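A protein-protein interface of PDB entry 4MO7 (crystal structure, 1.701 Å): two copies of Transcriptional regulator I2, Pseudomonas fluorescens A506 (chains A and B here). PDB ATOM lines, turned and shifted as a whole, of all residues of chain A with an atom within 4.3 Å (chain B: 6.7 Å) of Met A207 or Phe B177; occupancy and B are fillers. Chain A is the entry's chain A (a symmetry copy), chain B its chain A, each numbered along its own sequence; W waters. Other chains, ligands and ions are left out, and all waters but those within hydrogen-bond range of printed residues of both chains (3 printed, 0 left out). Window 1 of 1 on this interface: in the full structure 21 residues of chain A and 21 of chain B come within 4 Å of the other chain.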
ATOM      1  N   ALA A 181       6.313  24.858 -32.731  1.00  0.00           N
ATOM      2  CA  ALA A 181       6.245  23.546 -32.052  1.00  0.00           C
ATOM      3  C   ALA A 181       4.962  22.841 -32.395  1.00  0.00           C
ATOM      4  O   ALA A 181       4.959  21.626 -32.592  1.00  0.00           O
ATOM      5  CB  ALA A 181       6.364  23.741 -30.500  1.00  0.00           C
ATOM      6  N   THR A 185       3.988  19.288 -35.475  1.00  0.00           N
ATOM      7  CA  THR A 185       3.378  18.029 -35.022  1.00  0.00           C
ATOM      8  C   THR A 185       2.828  17.237 -36.231  1.00  0.00           C
ATOM      9  O   THR A 185       2.680  16.022 -36.128  1.00  0.00           O
ATOM     10  CB  THR A 185       2.314  18.127 -33.920  1.00  0.00           C
ATOM     11  OG1 THR A 185       1.204  18.870 -34.362  1.00  0.00           O
ATOM     12  CG2 THR A 185       2.838  18.800 -32.659  1.00  0.00           C
ATOM     13  N   LEU A 200      -1.313  15.296 -26.354  1.00  0.00           N
ATOM     14  CA  LEU A 200      -0.346  16.178 -27.040  1.00  0.00           C
ATOM     15  C   LEU A 200      -0.505  17.631 -26.553  1.00  0.00           C
ATOM     16  O   LEU A 200       0.485  18.331 -26.264  1.00  0.00           O
ATOM     17  CB  LEU A 200      -0.543  16.072 -28.559  1.00  0.00           C
ATOM     18  CG  LEU A 200       0.426  16.865 -29.460  1.00  0.00           C
ATOM     19  CD1 LEU A 200       1.890  16.352 -29.313  1.00  0.00           C
ATOM     20  CD2 LEU A 200      -0.021  16.837 -30.912  1.00  0.00           C
ATOM     21  N   GLU A 203       0.901  18.010 -23.099  1.00  0.00           N
ATOM     22  CA  GLU A 203       2.362  18.040 -23.115  1.00  0.00           C
ATOM     23  C   GLU A 203       2.794  19.418 -23.564  1.00  0.00           C
ATOM     24  O   GLU A 203       3.720  19.959 -22.984  1.00  0.00           O
ATOM     25  CB  GLU A 203       2.959  16.992 -24.041  1.00  0.00           C
ATOM     26  CG  GLU A 203       2.933  15.599 -23.524  1.00  0.00           C
ATOM     27  CD  GLU A 203       3.907  15.378 -22.349  1.00  0.00           C
ATOM     28  OE1 GLU A 203       5.012  16.012 -22.300  1.00  0.00           O
ATOM     29  OE2 GLU A 203       3.534  14.542 -21.489  1.00  0.00           O
ATOM     30  N   ALA A 204       2.108  20.014 -24.549  1.00  0.00           N
ATOM     31  CA  ALA A 204       2.463  21.402 -24.936  1.00  0.00           C
ATOM     32  C   ALA A 204       2.295  22.409 -23.816  1.00  0.00           C
ATOM     33  O   ALA A 204       3.106  23.312 -23.666  1.00  0.00           O
ATOM     34  CB  ALA A 204       1.688  21.908 -26.213  1.00  0.00           C
ATOM     35  N   LEU A 205       1.272  22.206 -22.995  1.00  0.00           N
ATOM     36  CA  LEU A 205       1.025  23.081 -21.869  1.00  0.00           C
ATOM     37  C   LEU A 205       2.143  22.952 -20.850  1.00  0.00           C
ATOM     38  O   LEU A 205       2.508  23.933 -20.244  1.00  0.00           O
ATOM     39  CB  LEU A 205      -0.304  22.679 -21.191  1.00  0.00           C
ATOM     40  CG  LEU A 205      -0.762  23.625 -20.097  1.00  0.00           C
ATOM     41  CD1 LEU A 205      -1.261  24.940 -20.738  1.00  0.00           C
ATOM     42  CD2 LEU A 205      -1.915  22.955 -19.351  1.00  0.00           C
ATOM     43  N   LEU A 206       2.645  21.730 -20.665  1.00  0.00           N
ATOM     44  CA  LEU A 206       3.743  21.469 -19.688  1.00  0.00           C
ATOM     45  C   LEU A 206       4.982  22.166 -20.143  1.00  0.00           C
ATOM     46  O   LEU A 206       5.751  22.706 -19.348  1.00  0.00           O
ATOM     47  CB  LEU A 206       4.031  19.985 -19.567  1.00  0.00           C
ATOM     48  CG  LEU A 206       3.087  19.094 -18.764  1.00  0.00           C
ATOM     49  CD1 LEU A 206       3.463  17.677 -19.016  1.00  0.00           C
ATOM     50  CD2 LEU A 206       3.196  19.371 -17.295  1.00  0.00           C
ATOM     51  N   MET A 207       5.192  22.177 -21.445  1.00  0.00           N
ATOM     52  CA  MET A 207       6.344  22.932 -21.913  1.00  0.00           C
ATOM     53  C   MET A 207       6.207  24.442 -21.719  1.00  0.00           C
ATOM     54  O   MET A 207       7.121  25.084 -21.212  1.00  0.00           O
ATOM     55  CB  MET A 207       6.659  22.640 -23.372  1.00  0.00           C
ATOM     56  CG  MET A 207       7.819  23.474 -23.827  1.00  0.00           C
ATOM     57  SD  MET A 207       8.201  23.063 -25.515  1.00  0.00           S
ATOM     58  CE  MET A 207       6.856  23.910 -26.371  1.00  0.00           C
ATOM     59  N   VAL A 208       5.075  25.021 -22.101  1.00  0.00           N
ATOM     60  CA  VAL A 208       5.006  26.448 -22.149  1.00  0.00           C
ATOM     61  C   VAL A 208       4.740  27.151 -20.792  1.00  0.00           C
ATOM     62  O   VAL A 208       5.195  28.265 -20.576  1.00  0.00           O
ATOM     63  CB  VAL A 208       4.134  26.933 -23.278  1.00  0.00           C
ATOM     64  CG1 VAL A 208       2.726  26.714 -22.964  1.00  0.00           C
ATOM     65  CG2 VAL A 208       4.388  28.396 -23.527  1.00  0.00           C
ATOM     66  N   LEU A 209       4.087  26.470 -19.858  1.00  0.00           N
ATOM     67  CA  LEU A 209       3.764  27.077 -18.571  1.00  0.00           C
ATOM     68  C   LEU A 209       4.752  26.568 -17.508  1.00  0.00           C
ATOM     69  O   LEU A 209       5.224  25.407 -17.580  1.00  0.00           O
ATOM     70  CB  LEU A 209       2.324  26.732 -18.147  1.00  0.00           C
ATOM     71  CG  LEU A 209       1.222  27.349 -19.031  1.00  0.00           C
ATOM     72  CD1 LEU A 209      -0.131  27.314 -18.338  1.00  0.00           C
ATOM     73  CD2 LEU A 209       1.562  28.787 -19.332  1.00  0.00           C
ATOM     74  N   ARG B 168       9.396  19.642 -17.304  1.00  0.00           N
ATOM     75  CA  ARG B 168       8.116  19.222 -16.733  1.00  0.00           C
ATOM     76  C   ARG B 168       7.541  18.033 -17.478  1.00  0.00           C
ATOM     77  O   ARG B 168       6.947  17.138 -16.853  1.00  0.00           O
ATOM     78  CB  ARG B 168       7.102  20.387 -16.767  1.00  0.00           C
ATOM     79  CG  ARG B 168       7.640  21.705 -16.224  1.00  0.00           C
ATOM     80  CD  ARG B 168       6.499  22.723 -16.105  1.00  0.00           C
ATOM     81  NE  ARG B 168       5.472  22.143 -15.263  1.00  0.00           N
ATOM     82  CZ  ARG B 168       4.166  22.281 -15.438  1.00  0.00           C
ATOM     83  NH1 ARG B 168       3.684  23.050 -16.417  1.00  0.00           N
ATOM     84  NH2 ARG B 168       3.333  21.663 -14.600  1.00  0.00           N
ATOM     85  N   GLY B 169       7.710  18.026 -18.798  1.00  0.00           N
ATOM     86  CA  GLY B 169       7.041  17.037 -19.648  1.00  0.00           C
ATOM     87  C   GLY B 169       7.881  15.831 -20.086  1.00  0.00           C
ATOM     88  O   GLY B 169       8.959  15.560 -19.538  1.00  0.00           O
ATOM     89  N   ASP B 170       7.362  15.097 -21.057  1.00  0.00           N
ATOM     90  CA  ASP B 170       8.051  13.915 -21.587  1.00  0.00           C
ATOM     91  C   ASP B 170       9.271  14.333 -22.421  1.00  0.00           C
ATOM     92  O   ASP B 170       9.242  15.337 -23.201  1.00  0.00           O
ATOM     93  CB  ASP B 170       7.046  13.146 -22.432  1.00  0.00           C
ATOM     94  CG  ASP B 170       7.641  11.943 -23.051  1.00  0.00           C
ATOM     95  OD1 ASP B 170       8.221  12.051 -24.153  1.00  0.00           O
ATOM     96  OD2 ASP B 170       7.507  10.874 -22.419  1.00  0.00           O
ATOM     97  N   PHE B 172      10.987  12.926 -24.877  1.00  0.00           N
ATOM     98  CA  PHE B 172      10.992  12.771 -26.305  1.00  0.00           C
ATOM     99  C   PHE B 172      10.075  13.793 -26.924  1.00  0.00           C
ATOM    100  O   PHE B 172      10.400  14.320 -27.990  1.00  0.00           O
ATOM    101  CB  PHE B 172      10.443  11.409 -26.689  1.00  0.00           C
ATOM    102  CG  PHE B 172      11.231  10.277 -26.069  1.00  0.00           C
ATOM    103  CD1 PHE B 172      12.395   9.866 -26.677  1.00  0.00           C
ATOM    104  CD2 PHE B 172      10.824   9.693 -24.864  1.00  0.00           C
ATOM    105  CE1 PHE B 172      13.162   8.839 -26.127  1.00  0.00           C
ATOM    106  CE2 PHE B 172      11.588   8.656 -24.297  1.00  0.00           C
ATOM    107  CZ  PHE B 172      12.763   8.265 -24.910  1.00  0.00           C
ATOM    108  N   ILE B 173       8.953  14.062 -26.265  1.00  0.00           N
ATOM    109  CA  ILE B 173       7.952  14.996 -26.836  1.00  0.00           C
ATOM    110  C   ILE B 173       8.518  16.423 -26.694  1.00  0.00           C
ATOM    111  O   ILE B 173       8.374  17.253 -27.609  1.00  0.00           O
ATOM    112  CB  ILE B 173       6.551  14.860 -26.187  1.00  0.00           C
ATOM    113  CG1 ILE B 173       5.950  13.450 -26.487  1.00  0.00           C
ATOM    114  CG2 ILE B 173       5.599  16.010 -26.712  1.00  0.00           C
ATOM    115  CD1 ILE B 173       6.345  12.840 -27.792  1.00  0.00           C
ATOM    116  N   THR B 174       9.210  16.682 -25.590  1.00  0.00           N
ATOM    117  CA  THR B 174       9.858  17.993 -25.402  1.00  0.00           C
ATOM    118  C   THR B 174      10.815  18.214 -26.577  1.00  0.00           C
ATOM    119  O   THR B 174      10.878  19.314 -27.175  1.00  0.00           O
ATOM    120  CB  THR B 174      10.618  18.073 -24.088  1.00  0.00           C
ATOM    121  OG1 THR B 174       9.676  18.001 -23.020  1.00  0.00           O
ATOM    122  CG2 THR B 174      11.364  19.402 -23.976  1.00  0.00           C
ATOM    123  N   ARG B 175      11.553  17.162 -26.965  1.00  0.00           N
ATOM    124  CA  ARG B 175      12.471  17.364 -28.098  1.00  0.00           C
ATOM    125  C   ARG B 175      11.717  17.617 -29.425  1.00  0.00           C
ATOM    126  O   ARG B 175      12.105  18.513 -30.204  1.00  0.00           O
ATOM    127  CB  ARG B 175      13.420  16.158 -28.228  1.00  0.00           C
ATOM    128  CG  ARG B 175      14.286  16.147 -29.513  1.00  0.00           C
ATOM    129  CD  ARG B 175      15.203  17.428 -29.582  1.00  0.00           C
ATOM    130  NE  ARG B 175      15.879  17.385 -30.915  1.00  0.00           N
ATOM    131  CZ  ARG B 175      16.357  18.445 -31.567  1.00  0.00           C
ATOM    132  NH1 ARG B 175      16.217  19.682 -31.053  1.00  0.00           N
ATOM    133  NH2 ARG B 175      16.862  18.278 -32.782  1.00  0.00           N
ATOM    134  N   ARG B 176      10.614  16.880 -29.664  1.00  0.00           N
ATOM    135  CA  ARG B 176       9.810  17.100 -30.873  1.00  0.00           C
ATOM    136  C   ARG B 176       9.286  18.563 -30.922  1.00  0.00           C
ATOM    137  O   ARG B 176       9.280  19.167 -31.979  1.00  0.00           O
ATOM    138  CB  ARG B 176       8.605  16.207 -30.871  1.00  0.00           C
ATOM    139  CG  ARG B 176       8.905  14.696 -30.770  1.00  0.00           C
ATOM    140  CD  ARG B 176       9.362  14.225 -32.073  1.00  0.00           C
ATOM    141  NE  ARG B 176       9.262  12.753 -32.130  1.00  0.00           N
ATOM    142  CZ  ARG B 176       9.448  12.069 -33.253  1.00  0.00           C
ATOM    143  NH1 ARG B 176       9.355  10.743 -33.274  1.00  0.00           N
ATOM    144  NH2 ARG B 176       9.731  12.730 -34.360  1.00  0.00           N
ATOM    145  N   PHE B 177       8.851  19.107 -29.792  1.00  0.00           N
ATOM    146  CA  PHE B 177       8.299  20.494 -29.793  1.00  0.00           C
ATOM    147  C   PHE B 177       9.452  21.450 -30.025  1.00  0.00           C
ATOM    148  O   PHE B 177       9.339  22.420 -30.769  1.00  0.00           O
ATOM    149  CB  PHE B 177       7.706  20.819 -28.396  1.00  0.00           C
ATOM    150  CG  PHE B 177       6.307  20.217 -28.117  1.00  0.00           C
ATOM    151  CD1 PHE B 177       5.383  19.987 -29.110  1.00  0.00           C
ATOM    152  CD2 PHE B 177       5.960  19.898 -26.807  1.00  0.00           C
ATOM    153  CE1 PHE B 177       4.074  19.424 -28.809  1.00  0.00           C
ATOM    154  CE2 PHE B 177       4.704  19.378 -26.471  1.00  0.00           C
ATOM    155  CZ  PHE B 177       3.769  19.111 -27.458  1.00  0.00           C
ATOM    156  N   LEU B 178      10.579  21.229 -29.362  1.00  0.00           N
ATOM    157  CA  LEU B 178      11.736  22.118 -29.537  1.00  0.00           C
ATOM    158  C   LEU B 178      12.298  22.089 -30.961  1.00  0.00           C
ATOM    159  O   LEU B 178      12.678  23.137 -31.546  1.00  0.00           O
ATOM    160  CB  LEU B 178      12.830  21.766 -28.480  1.00  0.00           C
ATOM    161  CG  LEU B 178      13.964  22.747 -28.244  1.00  0.00           C
ATOM    162  CD1 LEU B 178      13.460  24.148 -27.809  1.00  0.00           C
ATOM    163  CD2 LEU B 178      14.923  22.140 -27.200  1.00  0.00           C
ATOM    164  N   THR B 179      12.240  20.909 -31.586  1.00  0.00           N
ATOM    165  CA  THR B 179      12.658  20.783 -32.998  1.00  0.00           C
ATOM    166  C   THR B 179      11.833  21.747 -33.849  1.00  0.00           C
ATOM    167  O   THR B 179      12.384  22.500 -34.661  1.00  0.00           O
ATOM    168  CB  THR B 179      12.511  19.343 -33.515  1.00  0.00           C
ATOM    169  OG1 THR B 179      13.371  18.492 -32.733  1.00  0.00           O
ATOM    170  CG2 THR B 179      13.035  19.295 -34.910  1.00  0.00           C
ATOM    171  N   GLY B 180      10.517  21.722 -33.656  1.00  0.00           N
ATOM    172  CA  GLY B 180       9.620  22.570 -34.443  1.00  0.00           C
ATOM    173  C   GLY B 180       9.782  24.041 -34.099  1.00  0.00           C
ATOM    174  O   GLY B 180       9.711  24.930 -34.988  1.00  0.00           O
ATOM    175  N   ALA B 181       9.961  24.329 -32.813  1.00  0.00           N
ATOM    176  CA  ALA B 181      10.069  25.744 -32.396  1.00  0.00           C
ATOM    177  C   ALA B 181      11.320  26.365 -32.955  1.00  0.00           C
ATOM    178  O   ALA B 181      11.300  27.522 -33.374  1.00  0.00           O
ATOM    179  CB  ALA B 181      10.063  25.842 -30.830  1.00  0.00           C
ATOM    180  N   LEU B 182      12.429  25.622 -32.935  1.00  0.00           N
ATOM    181  CA  LEU B 182      13.707  26.176 -33.457  1.00  0.00           C
ATOM    182  C   LEU B 182      13.704  26.264 -34.978  1.00  0.00           C
ATOM    183  O   LEU B 182      14.160  27.284 -35.548  1.00  0.00           O
ATOM    184  CB  LEU B 182      14.927  25.323 -32.977  1.00  0.00           C
ATOM    185  CG  LEU B 182      15.097  25.309 -31.447  1.00  0.00           C
ATOM    186  CD1 LEU B 182      16.424  24.660 -30.989  1.00  0.00           C
ATOM    187  CD2 LEU B 182      15.118  26.753 -30.834  1.00  0.00           C
ATOM    188  N   LEU B 206      14.461  29.619 -21.831  1.00  0.00           N
ATOM    189  CA  LEU B 206      13.433  30.064 -20.844  1.00  0.00           C
ATOM    190  C   LEU B 206      12.170  29.303 -21.072  1.00  0.00           C
ATOM    191  O   LEU B 206      11.462  28.926 -20.137  1.00  0.00           O
ATOM    192  CB  LEU B 206      13.145  31.547 -20.980  1.00  0.00           C
ATOM    193  CG  LEU B 206      14.137  32.566 -20.425  1.00  0.00           C
ATOM    194  CD1 LEU B 206      13.735  33.914 -20.909  1.00  0.00           C
ATOM    195  CD2 LEU B 206      14.135  32.567 -18.927  1.00  0.00           C
ATOM    196  N   MET B 207      11.867  29.052 -22.331  1.00  0.00           N
ATOM    197  CA  MET B 207      10.689  28.231 -22.567  1.00  0.00           C
ATOM    198  C   MET B 207      10.850  26.783 -22.106  1.00  0.00           C
ATOM    199  O   MET B 207       9.979  26.253 -21.424  1.00  0.00           O
ATOM    200  CB  MET B 207      10.269  28.249 -24.028  1.00  0.00           C
ATOM    201  CG  MET B 207       9.085  27.354 -24.237  1.00  0.00           C
ATOM    202  SD  MET B 207       8.581  27.446 -25.940  1.00  0.00           S
ATOM    203  CE  MET B 207       9.868  26.445 -26.718  1.00  0.00           C
ATOM    204  N   VAL B 208      11.956  26.135 -22.453  1.00  0.00           N
ATOM    205  CA  VAL B 208      12.031  24.724 -22.240  1.00  0.00           C
ATOM    206  C   VAL B 208      12.398  24.283 -20.799  1.00  0.00           C
ATOM    207  O   VAL B 208      11.967  23.232 -20.348  1.00  0.00           O
ATOM    208  CB  VAL B 208      12.823  24.032 -23.319  1.00  0.00           C
ATOM    209  CG1 VAL B 208      14.249  24.295 -23.152  1.00  0.00           C
ATOM    210  CG2 VAL B 208      12.563  22.550 -23.274  1.00  0.00           C
ATOM    211  N   LEU B 209      13.111  25.121 -20.057  1.00  0.00           N
ATOM    212  CA  LEU B 209      13.530  24.762 -18.706  1.00  0.00           C
ATOM    213  C   LEU B 209      12.617  25.466 -17.688  1.00  0.00           C
ATOM    214  O   LEU B 209      12.133  26.597 -17.941  1.00  0.00           O
ATOM    215  CB  LEU B 209      14.994  25.170 -18.457  1.00  0.00           C
ATOM    216  CG  LEU B 209      16.033  24.392 -19.288  1.00  0.00           C
ATOM    217  CD1 LEU B 209      17.433  24.546 -18.712  1.00  0.00           C
ATOM    218  CD2 LEU B 209      15.683  22.926 -19.292  1.00  0.00           C
HETATM  219  O   HOH W   1       6.331  18.896 -22.631  1.00  0.00           O
HETATM  220  O   HOH W   2       8.637  25.891 -18.906  1.00  0.00           O
HETATM  221  O   HOH W   3       6.494  19.314 -32.656  1.00  0.00           O
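N of Asp B170 sits at hydrogen-bond distance from OE1 of Glu A203 (2.8 Å).
O of Met A207 lies close to O of Met B207.
O of Leu A209 sits at hydrogen-bond distance from NH1 of Arg B168.
Water W3 bridges the backbone carbonyl oxygen (O) of Ala A181 (2.8 Å) and the backbone carbonyl oxygen (O) of Arg B176 (2.9 Å).
Water W1 bridges O of Glu A203 (2.8 Å) and OG1 of Thr B174 (3.5 Å).
Water W2 lies within hydrogen-bond range of the backbone carbonyl oxygen of Met A207 (2.9 Å) and the backbone carbonyl oxygen of Met B207 (2.9 Å).
The side-chain carboxylate of Asp B170 lies within hydrogen-bond range of the backbone NH of Phe B172, at 3.0 Å.
OG1 of Thr B174 sits at hydrogen-bond distance from O of Asp B170 (2.7 Å).
The side-chain carboxylate (OD1) of Asp B170 sits at hydrogen-bond distance from the backbone NH (N) of Ile B173 (3.0 Å).
Of the printed residues of chain B, Leu A200 touches Phe B177 (3.6 Å).
Met A207 touches just these residues of chain B: Phe B177 and Met B207.
Printed residues of chain A within 4 Å of Arg B168: Leu A206 (3.3 Å) and Leu A209 (3.0 Å).
Phe B177 touches five residues of chain A.
Leu B209 touches none of the printed residues of chain A.
The nearest printed residue of chain A that does not touch Ala B181 is Met A207 (5.8 Å).
Hydrophobic or aromatic side chains of chain B within 4 Å of the printed part of chain A: Ile B173, Phe B177 and Met B207.
Of the 10 printed residues of chain A, 7 touch a printed residue of chain B.
Printed residues of chain A that touch a printed residue of chain B: Ala A181, Leu A200, Glu A203, Ala A204, Leu A206, Met A207 and Leu A209.
Hydrophobic or aromatic side chains of chain A within 4 Å of the printed part of chain B: Ala A181, Leu A200, Ala A204, Leu A206 and Met A207.
O of Phe B177 touches CB of Ala A181, 3.3 Å away.
Ala A181 touches Gly B180.
Ala A181 touches Ala B181.
Glu A203 touches Gly B169 (OE1 to CA, 3.5 Å).
Ile B173 touches Glu A203 (CG2 to CB, 3.9 Å).
C of Glu A203 touches CE2 of Phe B177, at 3.5 Å.
Ala A204 touches Phe B177.
Arg B168 touches Leu A206.
CD1 of Leu A206 touches CA of Gly B169 (3.7 Å).
Phe B177 touches Met A207 (CB to SD, 3.7 Å).
Ala A181 touches its own counterpart, Ala B181.
Met B207 touches its own counterpart, Met A207.
Of the 14 pairs that touch across the chains among the printed residues, 2 have their exchanged pair printed and touching as well.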
